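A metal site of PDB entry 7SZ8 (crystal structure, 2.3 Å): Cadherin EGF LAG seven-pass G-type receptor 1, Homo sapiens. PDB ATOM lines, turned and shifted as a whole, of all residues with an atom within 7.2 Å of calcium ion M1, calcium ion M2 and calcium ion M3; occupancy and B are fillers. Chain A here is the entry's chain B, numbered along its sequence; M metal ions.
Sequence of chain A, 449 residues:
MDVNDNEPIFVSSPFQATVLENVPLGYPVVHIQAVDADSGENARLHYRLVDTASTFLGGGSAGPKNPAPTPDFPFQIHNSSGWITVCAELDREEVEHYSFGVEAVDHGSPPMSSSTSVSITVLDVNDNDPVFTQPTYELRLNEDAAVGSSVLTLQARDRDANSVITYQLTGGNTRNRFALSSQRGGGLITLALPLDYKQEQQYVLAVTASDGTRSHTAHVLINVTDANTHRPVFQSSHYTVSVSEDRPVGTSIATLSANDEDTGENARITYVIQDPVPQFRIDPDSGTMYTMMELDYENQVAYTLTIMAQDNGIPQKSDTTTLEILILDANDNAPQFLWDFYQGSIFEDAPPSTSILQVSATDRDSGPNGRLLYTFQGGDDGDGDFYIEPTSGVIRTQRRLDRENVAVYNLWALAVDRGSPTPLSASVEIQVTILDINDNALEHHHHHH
OD2 of Asp 158 binds calcium ion M1, 2.2 Å away. Calcium ion M1 is bound by O of Asn 128. Calcium ion M1 is bound by OD2 of Asp 211 (2.3 Å). Calcium ion M1 is bound by OD1 of Asn 126, at 2.4 Å. Calcium ion M1 is bound by OD2 of Asp 160 (2.5 Å). The side-chain carboxylate (OD1) of Asp 158 binds calcium ion M1. Calcium ion M1 has six donor atoms within binding distance.
Five residues have an atom within 4 Å of calcium ion M1: Asn 126, Asn 128, Asp 158, Asp 160 and Asp 211. The nearest printed residue that does not touch calcium ion M1 is Asp 129 (4.5 Å).
The backbone carbonyl oxygen (O) of Leu 123 sits at hydrogen-bond distance from the backbone NH (N) of Glu 21. The side-chain carboxylate of Asp 127 sits close to the side-chain amide nitrogen of Asn 128, 3.2 Å away. The side-chain carboxylate (OE2) of Glu 93 lies close to the side-chain amide nitrogen (ND2) of Asn 128 (3.4 Å). The side-chain amide oxygen of Asn 128 sits at hydrogen-bond distance from the guanidinium group of Arg 159 (3.3 Å). N of Thr 213 sits at hydrogen-bond distance from OD1 of Asp 211 (3.1 Å). OE1 of Glu 93 lies close to NH2 of Arg 92, at 2.8 Å. O of Asn 126 is in hydrogen-bond range of NE of Arg 214 (3.1 Å). The guanidinium group (NE) of Arg 92 lies close to the side-chain carboxylate (OD1) of Asp 124, 3.2 Å away.
Within 4 Å of calcium ion M3: Glu 21, Asp 91, Glu 93 and Asp 127.
Within 4 Å of calcium ion M2: Glu 21, Glu 93, Asp 124, Val 125, Asp 127 and Asp 160.
Calcium ion M3 is bound by the side-chain carboxylate of Glu 21, the side-chain carboxylate of Asp 127, the side-chain carboxylate of Glu 93 and the side-chain carboxylate of Asp 91. Slightly farther from calcium ion M3 lies OD1 of Asp 127 (3.1 Å).
Calcium ion M2 is bound by OD1 of Asp 160 (2.2 Å), O of Val 125 (2.3 Å), OE1 of Glu 93 (2.3 Å), OD1 of Asp 124 (2.4 Å), OD1 of Asp 127 (2.5 Å), OE1 of Glu 21 (2.6 Å) and OE2 of Glu 93 (2.7 Å).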
ATOM      1  N   GLU A  21       1.971  -7.308 -10.811  1.00  0.00           N
ATOM      2  CA  GLU A  21       2.615  -6.011 -10.437  1.00  0.00           C
ATOM      3  C   GLU A  21       3.204  -6.063  -9.023  1.00  0.00           C
ATOM      4  O   GLU A  21       4.028  -5.180  -8.726  1.00  0.00           O
ATOM      5  CB  GLU A  21       1.624  -4.862 -10.596  1.00  0.00           C
ATOM      6  CG  GLU A  21       0.449  -4.871  -9.629  1.00  0.00           C
ATOM      7  CD  GLU A  21      -0.335  -3.573  -9.739  1.00  0.00           C
ATOM      8  OE1 GLU A  21      -1.414  -3.601 -10.340  1.00  0.00           O
ATOM      9  OE2 GLU A  21       0.179  -2.529  -9.277  1.00  0.00           O
ATOM     10  N   ASN A  22       2.852  -7.094  -8.235  1.00  0.00           N
ATOM     11  CA  ASN A  22       3.187  -7.266  -6.787  1.00  0.00           C
ATOM     12  C   ASN A  22       4.216  -8.392  -6.564  1.00  0.00           C
ATOM     13  O   ASN A  22       4.252  -8.948  -5.431  1.00  0.00           O
ATOM     14  CB  ASN A  22       1.913  -7.588  -6.013  1.00  0.00           C
ATOM     15  CG  ASN A  22       1.413  -8.979  -6.332  1.00  0.00           C
ATOM     16  OD1 ASN A  22       1.804  -9.565  -7.337  1.00  0.00           O
ATOM     17  ND2 ASN A  22       0.588  -9.547  -5.463  1.00  0.00           N
ATOM     18  N   LEU A  90       7.222  -3.402  -9.333  1.00  0.00           N
ATOM     19  CA  LEU A  90       6.416  -2.913 -10.475  1.00  0.00           C
ATOM     20  C   LEU A  90       5.178  -2.211  -9.930  1.00  0.00           C
ATOM     21  O   LEU A  90       4.995  -2.185  -8.694  1.00  0.00           O
ATOM     22  CB  LEU A  90       6.038  -4.083 -11.385  1.00  0.00           C
ATOM     23  CG  LEU A  90       7.232  -4.884 -11.920  1.00  0.00           C
ATOM     24  CD1 LEU A  90       6.757  -6.095 -12.701  1.00  0.00           C
ATOM     25  CD2 LEU A  90       8.133  -3.991 -12.764  1.00  0.00           C
ATOM     26  N   ASP A  91       4.372  -1.658 -10.827  1.00  0.00           N
ATOM     27  CA  ASP A  91       3.060  -1.039 -10.518  1.00  0.00           C
ATOM     28  C   ASP A  91       2.384  -0.732 -11.854  1.00  0.00           C
ATOM     29  O   ASP A  91       2.819   0.223 -12.512  1.00  0.00           O
ATOM     30  CB  ASP A  91       3.236   0.173  -9.588  1.00  0.00           C
ATOM     31  CG  ASP A  91       2.025   1.085  -9.468  1.00  0.00           C
ATOM     32  OD1 ASP A  91       0.887   0.656  -9.798  1.00  0.00           O
ATOM     33  OD2 ASP A  91       2.244   2.238  -9.041  1.00  0.00           O
ATOM     34  N   ARG A  92       1.369  -1.533 -12.221  1.00  0.00           N
ATOM     35  CA  ARG A  92       0.578  -1.403 -13.474  1.00  0.00           C
ATOM     36  C   ARG A  92       0.028   0.022 -13.630  1.00  0.00           C
ATOM     37  O   ARG A  92      -0.068   0.495 -14.781  1.00  0.00           O
ATOM     38  CB  ARG A  92      -0.574  -2.395 -13.488  1.00  0.00           C
ATOM     39  CG  ARG A  92      -1.227  -2.544 -14.854  1.00  0.00           C
ATOM     40  CD  ARG A  92      -2.647  -3.073 -14.821  1.00  0.00           C
ATOM     41  NE  ARG A  92      -3.470  -2.189 -14.030  1.00  0.00           N
ATOM     42  CZ  ARG A  92      -4.130  -1.124 -14.471  1.00  0.00           C
ATOM     43  NH1 ARG A  92      -4.102  -0.802 -15.757  1.00  0.00           N
ATOM     44  NH2 ARG A  92      -4.844  -0.401 -13.631  1.00  0.00           N
ATOM     45  N   GLU A  93      -0.313   0.682 -12.534  1.00  0.00           N
ATOM     46  CA  GLU A  93      -1.085   1.966 -12.569  1.00  0.00           C
ATOM     47  C   GLU A  93      -0.177   3.085 -13.113  1.00  0.00           C
ATOM     48  O   GLU A  93      -0.676   3.928 -13.907  1.00  0.00           O
ATOM     49  CB  GLU A  93      -1.696   2.264 -11.185  1.00  0.00           C
ATOM     50  CG  GLU A  93      -2.945   1.451 -10.876  1.00  0.00           C
ATOM     51  CD  GLU A  93      -2.783  -0.035 -10.586  1.00  0.00           C
ATOM     52  OE1 GLU A  93      -3.430  -0.834 -11.278  1.00  0.00           O
ATOM     53  OE2 GLU A  93      -2.047  -0.390  -9.622  1.00  0.00           O
ATOM     54  N   GLU A  94       1.092   3.061 -12.720  1.00  0.00           N
ATOM     55  CA  GLU A  94       2.183   3.946 -13.188  1.00  0.00           C
ATOM     56  C   GLU A  94       2.588   3.595 -14.631  1.00  0.00           C
ATOM     57  O   GLU A  94       2.539   4.490 -15.481  1.00  0.00           O
ATOM     58  CB  GLU A  94       3.341   3.800 -12.212  1.00  0.00           C
ATOM     59  CG  GLU A  94       4.397   4.874 -12.326  1.00  0.00           C
ATOM     60  CD  GLU A  94       5.445   4.756 -11.237  1.00  0.00           C
ATOM     61  OE1 GLU A  94       5.336   3.790 -10.444  1.00  0.00           O
ATOM     62  OE2 GLU A  94       6.346   5.631 -11.165  1.00  0.00           O
ATOM     63  N   LEU A 123       0.605  -7.370 -15.217  1.00  0.00           N
ATOM     64  CA  LEU A 123      -0.761  -7.875 -14.878  1.00  0.00           C
ATOM     65  C   LEU A 123      -1.292  -7.145 -13.621  1.00  0.00           C
ATOM     66  O   LEU A 123      -0.473  -6.777 -12.712  1.00  0.00           O
ATOM     67  CB  LEU A 123      -0.710  -9.386 -14.658  1.00  0.00           C
ATOM     68  CG  LEU A 123      -0.602 -10.238 -15.919  1.00  0.00           C
ATOM     69  CD1 LEU A 123      -0.174 -11.662 -15.563  1.00  0.00           C
ATOM     70  CD2 LEU A 123      -1.902 -10.263 -16.737  1.00  0.00           C
ATOM     71  N   ASP A 124      -2.615  -6.973 -13.572  1.00  0.00           N
ATOM     72  CA  ASP A 124      -3.298  -6.140 -12.548  1.00  0.00           C
ATOM     73  C   ASP A 124      -3.413  -6.902 -11.208  1.00  0.00           C
ATOM     74  O   ASP A 124      -3.600  -8.155 -11.235  1.00  0.00           O
ATOM     75  CB  ASP A 124      -4.707  -5.680 -12.968  1.00  0.00           C
ATOM     76  CG  ASP A 124      -5.243  -4.639 -12.017  1.00  0.00           C
ATOM     77  OD1 ASP A 124      -4.409  -3.856 -11.484  1.00  0.00           O
ATOM     78  OD2 ASP A 124      -6.478  -4.632 -11.756  1.00  0.00           O
ATOM     79  N   VAL A 125      -3.304  -6.147 -10.104  1.00  0.00           N
ATOM     80  CA  VAL A 125      -3.616  -6.499  -8.692  1.00  0.00           C
ATOM     81  C   VAL A 125      -4.658  -5.485  -8.180  1.00  0.00           C
ATOM     82  O   VAL A 125      -4.585  -4.289  -8.579  1.00  0.00           O
ATOM     83  CB  VAL A 125      -2.317  -6.493  -7.827  1.00  0.00           C
ATOM     84  CG1 VAL A 125      -2.562  -6.048  -6.382  1.00  0.00           C
ATOM     85  CG2 VAL A 125      -1.599  -7.830  -7.851  1.00  0.00           C
ATOM     86  N   ASN A 126      -5.556  -5.919  -7.287  1.00  0.00           N
ATOM     87  CA  ASN A 126      -6.477  -5.005  -6.548  1.00  0.00           C
ATOM     88  C   ASN A 126      -5.704  -4.375  -5.367  1.00  0.00           C
ATOM     89  O   ASN A 126      -5.869  -4.841  -4.248  1.00  0.00           O
ATOM     90  CB  ASN A 126      -7.756  -5.713  -6.128  1.00  0.00           C
ATOM     91  CG  ASN A 126      -8.804  -4.757  -5.590  1.00  0.00           C
ATOM     92  OD1 ASN A 126      -8.709  -3.547  -5.773  1.00  0.00           O
ATOM     93  ND2 ASN A 126      -9.832  -5.303  -4.970  1.00  0.00           N
ATOM     94  N   ASP A 127      -4.872  -3.370  -5.633  1.00  0.00           N
ATOM     95  CA  ASP A 127      -4.023  -2.675  -4.630  1.00  0.00           C
ATOM     96  C   ASP A 127      -4.514  -1.231  -4.459  1.00  0.00           C
ATOM     97  O   ASP A 127      -3.948  -0.536  -3.609  1.00  0.00           O
ATOM     98  CB  ASP A 127      -2.520  -2.747  -4.964  1.00  0.00           C
ATOM     99  CG  ASP A 127      -2.046  -2.360  -6.369  1.00  0.00           C
ATOM    100  OD1 ASP A 127      -2.905  -2.121  -7.269  1.00  0.00           O
ATOM    101  OD2 ASP A 127      -0.796  -2.298  -6.561  1.00  0.00           O
ATOM    102  N   ASN A 128      -5.589  -0.822  -5.157  1.00  0.00           N
ATOM    103  CA  ASN A 128      -6.201   0.530  -5.011  1.00  0.00           C
ATOM    104  C   ASN A 128      -7.622   0.442  -4.452  1.00  0.00           C
ATOM    105  O   ASN A 128      -8.436  -0.366  -4.959  1.00  0.00           O
ATOM    106  CB  ASN A 128      -6.216   1.304  -6.329  1.00  0.00           C
ATOM    107  CG  ASN A 128      -4.831   1.785  -6.709  1.00  0.00           C
ATOM    108  OD1 ASN A 128      -4.533   2.973  -6.644  1.00  0.00           O
ATOM    109  ND2 ASN A 128      -3.967   0.867  -7.113  1.00  0.00           N
ATOM    110  N   ASP A 129      -7.879   1.281  -3.445  1.00  0.00           N
ATOM    111  CA  ASP A 129      -9.216   1.627  -2.899  1.00  0.00           C
ATOM    112  C   ASP A 129      -9.908   2.554  -3.887  1.00  0.00           C
ATOM    113  O   ASP A 129      -9.213   3.418  -4.418  1.00  0.00           O
ATOM    114  CB  ASP A 129      -9.118   2.442  -1.610  1.00  0.00           C
ATOM    115  CG  ASP A 129      -8.652   1.681  -0.389  1.00  0.00           C
ATOM    116  OD1 ASP A 129      -8.578   0.425  -0.450  1.00  0.00           O
ATOM    117  OD2 ASP A 129      -8.373   2.353   0.623  1.00  0.00           O
ATOM    118  N   PRO A 130     -11.254   2.465  -4.068  1.00  0.00           N
ATOM    119  CA  PRO A 130     -12.015   3.558  -4.676  1.00  0.00           C
ATOM    120  C   PRO A 130     -11.658   4.903  -4.027  1.00  0.00           C
ATOM    121  O   PRO A 130     -11.470   4.921  -2.826  1.00  0.00           O
ATOM    122  CB  PRO A 130     -13.493   3.241  -4.397  1.00  0.00           C
ATOM    123  CG  PRO A 130     -13.527   1.733  -4.150  1.00  0.00           C
ATOM    124  CD  PRO A 130     -12.138   1.368  -3.644  1.00  0.00           C
ATOM    125  N   ARG A 157     -13.904   6.535  -8.342  1.00  0.00           N
ATOM    126  CA  ARG A 157     -13.186   5.849  -9.446  1.00  0.00           C
ATOM    127  C   ARG A 157     -12.139   4.977  -8.782  1.00  0.00           C
ATOM    128  O   ARG A 157     -11.873   5.207  -7.610  1.00  0.00           O
ATOM    129  CB  ARG A 157     -12.576   6.852 -10.438  1.00  0.00           C
ATOM    130  CG  ARG A 157     -13.616   7.609 -11.268  1.00  0.00           C
ATOM    131  CD  ARG A 157     -13.003   8.309 -12.470  1.00  0.00           C
ATOM    132  NE  ARG A 157     -13.625   9.606 -12.771  1.00  0.00           N
ATOM    133  CZ  ARG A 157     -13.063  10.592 -13.477  1.00  0.00           C
ATOM    134  NH1 ARG A 157     -11.845  10.459 -13.983  1.00  0.00           N
ATOM    135  NH2 ARG A 157     -13.718  11.727 -13.658  1.00  0.00           N
ATOM    136  N   ASP A 158     -11.632   3.989  -9.523  1.00  0.00           N
ATOM    137  CA  ASP A 158     -10.614   2.985  -9.098  1.00  0.00           C
ATOM    138  C   ASP A 158      -9.574   2.957 -10.214  1.00  0.00           C
ATOM    139  O   ASP A 158      -9.948   2.764 -11.381  1.00  0.00           O
ATOM    140  CB  ASP A 158     -11.267   1.620  -8.818  1.00  0.00           C
ATOM    141  CG  ASP A 158     -10.428   0.577  -8.089  1.00  0.00           C
ATOM    142  OD1 ASP A 158      -9.523   0.006  -8.702  1.00  0.00           O
ATOM    143  OD2 ASP A 158     -10.739   0.271  -6.937  1.00  0.00           O
ATOM    144  N   ARG A 159      -8.309   3.185  -9.860  1.00  0.00           N
ATOM    145  CA  ARG A 159      -7.162   3.215 -10.789  1.00  0.00           C
ATOM    146  C   ARG A 159      -6.798   1.786 -11.206  1.00  0.00           C
ATOM    147  O   ARG A 159      -6.104   1.641 -12.206  1.00  0.00           O
ATOM    148  CB  ARG A 159      -6.007   3.993 -10.143  1.00  0.00           C
ATOM    149  CG  ARG A 159      -6.303   5.474  -9.967  1.00  0.00           C
ATOM    150  CD  ARG A 159      -5.499   6.153  -8.881  1.00  0.00           C
ATOM    151  NE  ARG A 159      -4.240   6.663  -9.422  1.00  0.00           N
ATOM    152  CZ  ARG A 159      -3.065   6.037  -9.381  1.00  0.00           C
ATOM    153  NH1 ARG A 159      -2.932   4.858  -8.771  1.00  0.00           N
ATOM    154  NH2 ARG A 159      -2.012   6.612  -9.936  1.00  0.00           N
ATOM    155  N   ASP A 160      -7.277   0.759 -10.491  1.00  0.00           N
ATOM    156  CA  ASP A 160      -7.148  -0.643 -10.969  1.00  0.00           C
ATOM    157  C   ASP A 160      -8.043  -0.772 -12.210  1.00  0.00           C
ATOM    158  O   ASP A 160      -8.912   0.094 -12.431  1.00  0.00           O
ATOM    159  CB  ASP A 160      -7.477  -1.691  -9.914  1.00  0.00           C
ATOM    160  CG  ASP A 160      -6.638  -1.576  -8.658  1.00  0.00           C
ATOM    161  OD1 ASP A 160      -5.387  -1.426  -8.785  1.00  0.00           O
ATOM    162  OD2 ASP A 160      -7.235  -1.617  -7.556  1.00  0.00           O
ATOM    163  N   ALA A 161      -7.778  -1.806 -13.003  1.00  0.00           N
ATOM    164  CA  ALA A 161      -8.468  -2.060 -14.281  1.00  0.00           C
ATOM    165  C   ALA A 161      -9.805  -2.706 -13.991  1.00  0.00           C
ATOM    166  O   ALA A 161      -9.912  -3.376 -12.933  1.00  0.00           O
ATOM    167  CB  ALA A 161      -7.605  -2.940 -15.163  1.00  0.00           C
ATOM    168  N   SER A 163     -12.712  -2.372 -12.815  1.00  0.00           N
ATOM    169  CA  SER A 163     -13.295  -2.461 -11.462  1.00  0.00           C
ATOM    170  C   SER A 163     -14.745  -1.992 -11.537  1.00  0.00           C
ATOM    171  O   SER A 163     -15.070  -1.120 -12.357  1.00  0.00           O
ATOM    172  CB  SER A 163     -12.461  -1.735 -10.436  1.00  0.00           C
ATOM    173  OG  SER A 163     -12.954  -0.430 -10.287  1.00  0.00           O
ATOM    174  N   ILE A 165     -17.855  -0.549  -9.326  1.00  0.00           N
ATOM    175  CA  ILE A 165     -18.070   0.220  -8.071  1.00  0.00           C
ATOM    176  C   ILE A 165     -19.533   0.106  -7.658  1.00  0.00           C
ATOM    177  O   ILE A 165     -20.405   0.315  -8.497  1.00  0.00           O
ATOM    178  CB  ILE A 165     -17.654   1.703  -8.212  1.00  0.00           C
ATOM    179  CG1 ILE A 165     -16.226   1.834  -8.727  1.00  0.00           C
ATOM    180  CG2 ILE A 165     -17.841   2.447  -6.896  1.00  0.00           C
ATOM    181  CD1 ILE A 165     -15.269   0.868  -8.083  1.00  0.00           C
ATOM    182  N   ASP A 211     -15.254  -1.781  -4.449  1.00  0.00           N
ATOM    183  CA  ASP A 211     -14.953  -2.509  -5.699  1.00  0.00           C
ATOM    184  C   ASP A 211     -15.224  -3.995  -5.471  1.00  0.00           C
ATOM    185  O   ASP A 211     -14.773  -4.765  -6.267  1.00  0.00           O
ATOM    186  CB  ASP A 211     -13.515  -2.225  -6.161  1.00  0.00           C
ATOM    187  CG  ASP A 211     -12.420  -2.703  -5.210  1.00  0.00           C
ATOM    188  OD1 ASP A 211     -12.721  -3.492  -4.296  1.00  0.00           O
ATOM    189  OD2 ASP A 211     -11.302  -2.283  -5.396  1.00  0.00           O
ATOM    190  N   THR A 213     -14.136  -5.925  -2.942  1.00  0.00           N
ATOM    191  CA  THR A 213     -13.112  -6.342  -1.954  1.00  0.00           C
ATOM    192  C   THR A 213     -12.719  -5.140  -1.082  1.00  0.00           C
ATOM    193  O   THR A 213     -12.785  -5.256   0.135  1.00  0.00           O
ATOM    194  CB  THR A 213     -11.918  -6.964  -2.685  1.00  0.00           C
ATOM    195  OG1 THR A 213     -12.484  -7.998  -3.482  1.00  0.00           O
ATOM    196  CG2 THR A 213     -10.849  -7.535  -1.784  1.00  0.00           C
ATOM    197  N   ARG A 214     -12.336  -4.028  -1.700  1.00  0.00           N
ATOM    198  CA  ARG A 214     -11.854  -2.796  -1.020  1.00  0.00           C
ATOM    199  C   ARG A 214     -12.921  -1.707  -1.100  1.00  0.00           C
ATOM    200  O   ARG A 214     -13.715  -1.691  -2.035  1.00  0.00           O
ATOM    201  CB  ARG A 214     -10.598  -2.271  -1.690  1.00  0.00           C
ATOM    202  CG  ARG A 214      -9.301  -2.943  -1.271  1.00  0.00           C
ATOM    203  CD  ARG A 214      -8.207  -2.320  -2.111  1.00  0.00           C
ATOM    204  NE  ARG A 214      -7.023  -3.132  -1.964  1.00  0.00           N
ATOM    205  CZ  ARG A 214      -5.978  -2.860  -1.176  1.00  0.00           C
ATOM    206  NH1 ARG A 214      -5.912  -1.754  -0.456  1.00  0.00           N
ATOM    207  NH2 ARG A 214      -4.991  -3.736  -1.137  1.00  0.00           N
HETATM  208 CA    CA M   1      -9.533  -1.484  -6.567  1.00  0.00          CA
HETATM  209 CA    CA M   2      -3.685  -2.474  -9.629  1.00  0.00          CA
HETATM  210 CA    CA M   3      -0.260  -0.770  -8.064  1.00  0.00          CA
